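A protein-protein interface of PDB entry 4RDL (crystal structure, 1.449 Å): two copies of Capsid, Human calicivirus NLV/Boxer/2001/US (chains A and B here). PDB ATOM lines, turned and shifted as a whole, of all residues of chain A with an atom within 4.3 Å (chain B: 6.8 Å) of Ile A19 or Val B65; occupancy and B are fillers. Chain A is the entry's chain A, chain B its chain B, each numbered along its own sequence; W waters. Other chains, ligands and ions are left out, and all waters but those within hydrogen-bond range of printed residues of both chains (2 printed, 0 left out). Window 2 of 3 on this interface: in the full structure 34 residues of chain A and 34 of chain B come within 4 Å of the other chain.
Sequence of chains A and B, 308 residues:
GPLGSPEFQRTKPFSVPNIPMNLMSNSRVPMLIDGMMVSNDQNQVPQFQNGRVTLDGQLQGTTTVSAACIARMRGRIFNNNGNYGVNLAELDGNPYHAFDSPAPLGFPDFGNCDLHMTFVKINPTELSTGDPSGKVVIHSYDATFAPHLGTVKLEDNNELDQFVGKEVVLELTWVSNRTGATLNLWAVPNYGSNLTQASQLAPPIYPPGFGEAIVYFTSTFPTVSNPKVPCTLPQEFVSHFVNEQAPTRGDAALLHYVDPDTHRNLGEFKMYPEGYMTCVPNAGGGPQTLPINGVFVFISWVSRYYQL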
ATOM      1  N   PRO A  17     -25.962  11.962  -0.936  1.00  0.00           N
ATOM      2  CA  PRO A  17     -26.501  13.261  -0.534  1.00  0.00           C
ATOM      3  C   PRO A  17     -26.375  14.333  -1.613  1.00  0.00           C
ATOM      4  O   PRO A  17     -25.367  14.421  -2.324  1.00  0.00           O
ATOM      5  CB  PRO A  17     -25.651  13.633   0.684  1.00  0.00           C
ATOM      6  CG  PRO A  17     -25.212  12.324   1.244  1.00  0.00           C
ATOM      7  CD  PRO A  17     -24.988  11.442   0.040  1.00  0.00           C
ATOM      8  N   ASN A  18     -27.437  15.122  -1.711  1.00  0.00           N
ATOM      9  CA  ASN A  18     -27.538  16.312  -2.533  1.00  0.00           C
ATOM     10  C   ASN A  18     -27.157  17.513  -1.671  1.00  0.00           C
ATOM     11  O   ASN A  18     -27.963  18.427  -1.452  1.00  0.00           O
ATOM     12  CB  ASN A  18     -28.986  16.453  -2.999  1.00  0.00           C
ATOM     13  CG  ASN A  18     -29.207  17.649  -3.878  1.00  0.00           C
ATOM     14  OD1 ASN A  18     -28.351  18.007  -4.684  1.00  0.00           O
ATOM     15  ND2 ASN A  18     -30.370  18.278  -3.736  1.00  0.00           N
ATOM     16  N   ILE A  19     -25.939  17.458  -1.142  1.00  0.00           N
ATOM     17  CA  ILE A  19     -25.350  18.512  -0.320  1.00  0.00           C
ATOM     18  C   ILE A  19     -23.952  18.814  -0.849  1.00  0.00           C
ATOM     19  O   ILE A  19     -23.170  17.893  -1.105  1.00  0.00           O
ATOM     20  CB  ILE A  19     -25.194  18.053   1.145  1.00  0.00           C
ATOM     21  CG1 ILE A  19     -26.545  17.684   1.755  1.00  0.00           C
ATOM     22  CG2 ILE A  19     -24.513  19.134   1.990  1.00  0.00           C
ATOM     23  CD1 ILE A  19     -26.439  16.944   3.055  1.00  0.00           C
ATOM     24  N   PRO A  20     -23.617  20.103  -1.011  1.00  0.00           N
ATOM     25  CA  PRO A  20     -22.259  20.434  -1.457  1.00  0.00           C
ATOM     26  C   PRO A  20     -21.189  19.851  -0.542  1.00  0.00           C
ATOM     27  O   PRO A  20     -21.350  19.798   0.681  1.00  0.00           O
ATOM     28  CB  PRO A  20     -22.238  21.963  -1.416  1.00  0.00           C
ATOM     29  CG  PRO A  20     -23.666  22.354  -1.613  1.00  0.00           C
ATOM     30  CD  PRO A  20     -24.457  21.303  -0.871  1.00  0.00           C
ATOM     31  N   MET A  21     -20.088  19.420  -1.142  1.00  0.00           N
ATOM     32  CA  MET A  21     -19.048  18.722  -0.403  1.00  0.00           C
ATOM     33  C   MET A  21     -18.557  19.523   0.800  1.00  0.00           C
ATOM     34  O   MET A  21     -18.329  18.959   1.885  1.00  0.00           O
ATOM     35  CB  MET A  21     -17.870  18.384  -1.321  1.00  0.00           C
ATOM     36  CG  MET A  21     -16.826  17.504  -0.642  1.00  0.00           C
ATOM     37  SD  MET A  21     -15.404  17.123  -1.682  1.00  0.00           S
ATOM     38  CE  MET A  21     -14.638  18.742  -1.799  1.00  0.00           C
ATOM     39  N   LEU A  23     -20.012  21.519   2.726  1.00  0.00           N
ATOM     40  CA  LEU A  23     -20.959  21.635   3.832  1.00  0.00           C
ATOM     41  C   LEU A  23     -21.035  20.351   4.656  1.00  0.00           C
ATOM     42  O   LEU A  23     -21.716  20.311   5.675  1.00  0.00           O
ATOM     43  CB  LEU A  23     -22.362  22.000   3.339  1.00  0.00           C
ATOM     44  CG  LEU A  23     -22.489  23.339   2.607  1.00  0.00           C
ATOM     45  CD1 LEU A  23     -23.942  23.669   2.316  1.00  0.00           C
ATOM     46  CD2 LEU A  23     -21.835  24.443   3.402  1.00  0.00           C
ATOM     47  N   MET A  24     -20.351  19.302   4.211  1.00  0.00           N
ATOM     48  CA  MET A  24     -20.375  18.031   4.928  1.00  0.00           C
ATOM     49  C   MET A  24     -19.162  17.881   5.836  1.00  0.00           C
ATOM     50  O   MET A  24     -18.156  18.571   5.661  1.00  0.00           O
ATOM     51  CB  MET A  24     -20.483  16.852   3.954  1.00  0.00           C
ATOM     52  CG  MET A  24     -21.862  16.776   3.309  1.00  0.00           C
ATOM     53  SD  MET A  24     -22.084  15.378   2.200  1.00  0.00           S
ATOM     54  CE  MET A  24     -21.033  15.906   0.846  1.00  0.00           C
ATOM     55  N   VAL A 295     -21.416  19.088  -5.969  1.00  0.00           N
ATOM     56  CA  VAL A 295     -22.389  18.158  -5.417  1.00  0.00           C
ATOM     57  C   VAL A 295     -22.218  16.812  -6.107  1.00  0.00           C
ATOM     58  O   VAL A 295     -22.179  16.754  -7.333  1.00  0.00           O
ATOM     59  CB  VAL A 295     -23.830  18.673  -5.643  1.00  0.00           C
ATOM     60  CG1 VAL A 295     -24.840  17.637  -5.196  1.00  0.00           C
ATOM     61  CG2 VAL A 295     -24.048  19.995  -4.898  1.00  0.00           C
ATOM     62  N   LEU B  59     -32.936  26.875   5.269  1.00  0.00           N
ATOM     63  CA  LEU B  59     -32.265  27.142   6.532  1.00  0.00           C
ATOM     64  C   LEU B  59     -32.571  28.544   7.049  1.00  0.00           C
ATOM     65  O   LEU B  59     -32.752  29.472   6.265  1.00  0.00           O
ATOM     66  CB  LEU B  59     -30.757  26.978   6.359  1.00  0.00           C
ATOM     67  CG  LEU B  59     -30.275  25.570   6.020  1.00  0.00           C
ATOM     68  CD1 LEU B  59     -28.847  25.613   5.549  1.00  0.00           C
ATOM     69  CD2 LEU B  59     -30.406  24.679   7.241  1.00  0.00           C
ATOM     70  N   THR B  63     -28.375  28.323  11.463  1.00  0.00           N
ATOM     71  CA  THR B  63     -28.406  26.881  11.235  1.00  0.00           C
ATOM     72  C   THR B  63     -27.532  26.446  10.057  1.00  0.00           C
ATOM     73  O   THR B  63     -27.521  27.099   9.013  1.00  0.00           O
ATOM     74  CB  THR B  63     -29.864  26.410  11.069  1.00  0.00           C
ATOM     75  OG1 THR B  63     -30.594  26.816  12.228  1.00  0.00           O
ATOM     76  CG2 THR B  63     -29.961  24.886  10.898  1.00  0.00           C
ATOM     77  N   THR B  64     -26.796  25.358  10.267  1.00  0.00           N
ATOM     78  CA  THR B  64     -25.941  24.729   9.269  1.00  0.00           C
ATOM     79  C   THR B  64     -26.490  23.368   8.886  1.00  0.00           C
ATOM     80  O   THR B  64     -27.350  22.807   9.569  1.00  0.00           O
ATOM     81  CB  THR B  64     -24.499  24.464   9.822  1.00  0.00           C
ATOM     82  OG1 THR B  64     -24.575  23.686  11.032  1.00  0.00           O
ATOM     83  CG2 THR B  64     -23.794  25.752  10.121  1.00  0.00           C
ATOM     84  N   VAL B  65     -25.933  22.807   7.824  1.00  0.00           N
ATOM     85  CA  VAL B  65     -26.283  21.453   7.428  1.00  0.00           C
ATOM     86  C   VAL B  65     -25.678  20.437   8.406  1.00  0.00           C
ATOM     87  O   VAL B  65     -26.369  19.542   8.884  1.00  0.00           O
ATOM     88  CB  VAL B  65     -25.805  21.152   6.003  1.00  0.00           C
ATOM     89  CG1 VAL B  65     -26.055  19.692   5.660  1.00  0.00           C
ATOM     90  CG2 VAL B  65     -26.526  22.059   5.008  1.00  0.00           C
ATOM     91  N   SER B  66     -24.395  20.593   8.722  1.00  0.00           N
ATOM     92  CA  SER B  66     -23.670  19.578   9.478  1.00  0.00           C
ATOM     93  C   SER B  66     -23.632  19.803  10.992  1.00  0.00           C
ATOM     94  O   SER B  66     -23.433  20.924  11.464  1.00  0.00           O
ATOM     95  CB  SER B  66     -22.239  19.477   8.959  1.00  0.00           C
ATOM     96  OG  SER B  66     -21.541  18.438   9.625  1.00  0.00           O
ATOM     97  N   ALA B  67     -23.774  18.714  11.744  1.00  0.00           N
ATOM     98  CA  ALA B  67     -23.617  18.763  13.198  1.00  0.00           C
ATOM     99  C   ALA B  67     -22.196  19.182  13.588  1.00  0.00           C
ATOM    100  O   ALA B  67     -21.960  19.626  14.714  1.00  0.00           O
ATOM    101  CB  ALA B  67     -23.972  17.424  13.825  1.00  0.00           C
ATOM    102  N   ALA B  68     -21.250  19.034  12.663  1.00  0.00           N
ATOM    103  CA  ALA B  68     -19.865  19.424  12.924  1.00  0.00           C
ATOM    104  C   ALA B  68     -19.694  20.931  13.149  1.00  0.00           C
ATOM    105  O   ALA B  68     -18.655  21.371  13.649  1.00  0.00           O
ATOM    106  CB  ALA B  68     -18.939  18.943  11.796  1.00  0.00           C
ATOM    107  N   CYS B  69     -20.704  21.715  12.787  1.00  0.00           N
ATOM    108  CA  CYS B  69     -20.622  23.175  12.934  1.00  0.00           C
ATOM    109  C   CYS B  69     -21.294  23.712  14.194  1.00  0.00           C
ATOM    110  O   CYS B  69     -21.150  24.887  14.524  1.00  0.00           O
ATOM    111  CB  CYS B  69     -21.258  23.867  11.738  1.00  0.00           C
ATOM    112  SG  CYS B  69     -20.485  23.471  10.171  1.00  0.00           S
ATOM    113  N   LEU B 105     -22.547  31.124  10.621  1.00  0.00           N
ATOM    114  CA  LEU B 105     -23.267  29.860  10.762  1.00  0.00           C
ATOM    115  C   LEU B 105     -22.635  28.994  11.858  1.00  0.00           C
ATOM    116  O   LEU B 105     -21.406  28.956  12.000  1.00  0.00           O
ATOM    117  CB  LEU B 105     -23.318  29.103   9.431  1.00  0.00           C
ATOM    118  CG  LEU B 105     -23.961  29.867   8.272  1.00  0.00           C
ATOM    119  CD1 LEU B 105     -24.070  28.947   7.065  1.00  0.00           C
ATOM    120  CD2 LEU B 105     -25.337  30.419   8.666  1.00  0.00           C
ATOM    121  N   GLN B 235     -30.631  17.578  14.664  1.00  0.00           N
ATOM    122  CA  GLN B 235     -29.819  18.123  13.585  1.00  0.00           C
ATOM    123  C   GLN B 235     -30.019  17.346  12.286  1.00  0.00           C
ATOM    124  O   GLN B 235     -30.058  17.932  11.206  1.00  0.00           O
ATOM    125  CB  GLN B 235     -28.335  18.164  13.955  1.00  0.00           C
ATOM    126  CG  GLN B 235     -27.470  18.782  12.858  1.00  0.00           C
ATOM    127  CD  GLN B 235     -27.831  20.232  12.595  1.00  0.00           C
ATOM    128  OE1 GLN B 235     -28.302  20.934  13.491  1.00  0.00           O
ATOM    129  NE2 GLN B 235     -27.607  20.692  11.363  1.00  0.00           N
ATOM    130  N   GLU B 236     -30.135  16.026  12.387  1.00  0.00           N
ATOM    131  CA  GLU B 236     -30.253  15.205  11.187  1.00  0.00           C
ATOM    132  C   GLU B 236     -31.584  15.415  10.451  1.00  0.00           C
ATOM    133  O   GLU B 236     -31.671  15.152   9.259  1.00  0.00           O
ATOM    134  CB  GLU B 236     -29.969  13.727  11.481  1.00  0.00           C
ATOM    135  CG  GLU B 236     -28.479  13.413  11.733  1.00  0.00           C
ATOM    136  CD  GLU B 236     -27.982  13.814  13.130  1.00  0.00           C
ATOM    137  OE1 GLU B 236     -28.798  14.194  13.994  1.00  0.00           O
ATOM    138  OE2 GLU B 236     -26.761  13.735  13.371  1.00  0.00           O
ATOM    139  N   VAL B 238     -32.637  18.450  10.047  1.00  0.00           N
ATOM    140  CA  VAL B 238     -32.265  19.636   9.282  1.00  0.00           C
ATOM    141  C   VAL B 238     -31.586  19.246   7.973  1.00  0.00           C
ATOM    142  O   VAL B 238     -31.991  19.701   6.895  1.00  0.00           O
ATOM    143  CB  VAL B 238     -31.318  20.573  10.071  1.00  0.00           C
ATOM    144  CG1 VAL B 238     -30.874  21.748   9.199  1.00  0.00           C
ATOM    145  CG2 VAL B 238     -31.996  21.083  11.338  1.00  0.00           C
ATOM    146  N   SER B 239     -30.551  18.411   8.056  1.00  0.00           N
ATOM    147  CA  SER B 239     -29.831  18.018   6.847  1.00  0.00           C
ATOM    148  C   SER B 239     -30.727  17.193   5.928  1.00  0.00           C
ATOM    149  O   SER B 239     -30.613  17.274   4.712  1.00  0.00           O
ATOM    150  CB  SER B 239     -28.536  17.263   7.168  1.00  0.00           C
ATOM    151  OG  SER B 239     -28.752  16.186   8.064  1.00  0.00           O
ATOM    152  N   HIS B 240     -31.620  16.403   6.514  1.00  0.00           N
ATOM    153  CA  HIS B 240     -32.564  15.629   5.722  1.00  0.00           C
ATOM    154  C   HIS B 240     -33.441  16.554   4.875  1.00  0.00           C
ATOM    155  O   HIS B 240     -33.589  16.352   3.668  1.00  0.00           O
ATOM    156  CB  HIS B 240     -33.431  14.749   6.630  1.00  0.00           C
ATOM    157  CG  HIS B 240     -34.300  13.783   5.888  1.00  0.00           C
ATOM    158  ND1 HIS B 240     -33.815  12.613   5.347  1.00  0.00           N
ATOM    159  CD2 HIS B 240     -35.623  13.813   5.601  1.00  0.00           C
ATOM    160  CE1 HIS B 240     -34.803  11.960   4.761  1.00  0.00           C
ATOM    161  NE2 HIS B 240     -35.909  12.668   4.895  1.00  0.00           N
ATOM    162  N   VAL B 242     -32.920  19.732   4.063  1.00  0.00           N
ATOM    163  CA  VAL B 242     -32.086  20.456   3.113  1.00  0.00           C
ATOM    164  C   VAL B 242     -31.789  19.565   1.911  1.00  0.00           C
ATOM    165  O   VAL B 242     -31.842  20.009   0.763  1.00  0.00           O
ATOM    166  CB  VAL B 242     -30.766  20.938   3.751  1.00  0.00           C
ATOM    167  CG1 VAL B 242     -29.831  21.473   2.675  1.00  0.00           C
ATOM    168  CG2 VAL B 242     -31.046  22.001   4.818  1.00  0.00           C
ATOM    169  N   ASN B 243     -31.499  18.297   2.179  1.00  0.00           N
ATOM    170  CA  ASN B 243     -31.223  17.343   1.110  1.00  0.00           C
ATOM    171  C   ASN B 243     -32.429  17.099   0.196  1.00  0.00           C
ATOM    172  O   ASN B 243     -32.304  17.096  -1.029  1.00  0.00           O
ATOM    173  CB  ASN B 243     -30.760  16.013   1.694  1.00  0.00           C
ATOM    174  CG  ASN B 243     -30.155  15.110   0.649  1.00  0.00           C
ATOM    175  OD1 ASN B 243     -28.983  15.246   0.314  1.00  0.00           O
ATOM    176  ND2 ASN B 243     -30.954  14.195   0.113  1.00  0.00           N
HETATM  177  O   HOH W   1     -22.631  22.358   7.277  1.00  0.00           O
HETATM  178  O   HOH W   2     -30.095  20.226  -1.138  1.00  0.00           O
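Among the printed residues, pairs that only touch across the chains: Pro A17 with Asn B243 (3.3 Å), Ile A19 with Val B65 (3.8 Å), Ile A19 with Asn B243 (3.7 Å) and Leu A23 with Ser B66 (3.4 Å).
The side-chain hydroxyl of Thr B64 is in hydrogen-bond range of the backbone carbonyl oxygen of Ser B66 (3.0 Å).
The backbone carbonyl oxygen of Val B65 is in hydrogen-bond range of the side-chain amide nitrogen of Gln B235 (3.0 Å).
The side-chain hydroxyl (OG) of Ser B66 lies close to the backbone NH (N) of Ala B68 (3.1 Å).
Water W2 lies within hydrogen-bond range of O of Val B242 and O of Asn A18.
Water W1 lies within hydrogen-bond range of O of Leu A23 (2.8 Å), N of Ser B66 (2.9 Å), N of Val B65 (3.4 Å) and SG of Cys B69 (3.8 Å).
No position is printed for both chains.
Of the 5 pairs that touch across the chains among the printed residues, none has its exchanged pair printed and touching as well.
Ile A19 touches just these residues of chain B: Val B65 and Asn B243.
Of chain A, only Ile A19 (3.8 Å) comes within 4 Å of Val B65.
Of the printed residues of chain A, Ser B66 touches Leu A23.
Of the printed residues of chain B, Pro A17 touches Asn B243 (3.3 Å).
Of the printed residues of chain B, Asn A18 touches Asn B243 (2.6 Å).
Of the printed residues of chain A, Asn B243 touches Pro A17 (3.3 Å), Asn A18 (2.6 Å) and Ile A19 (3.7 Å).
Met A24 touches none of the printed residues of chain B.
Ser B239 touches none of the printed residues of chain A.
The nearest residue of chain A that does not touch Val B65 is Leu A23 (4.1 Å).
The nearest printed residue of chain B that does not touch Pro A17 is Ser B239 (7.4 Å).
Hydrophobic or aromatic side chains of chain A that line the printed part of chain B: Pro A17 and Ile A19.
Printed residues of chain B that touch a printed residue of chain A: Val B65, Ser B66 and Asn B243.
Among the printed residues, no Asp or Glu carboxylate lies within 4 Å of a Lys or Arg side-chain nitrogen of the other chain.
N of Asn A18 sits at hydrogen-bond distance from OD1 of Asn B243, 2.6 Å away.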
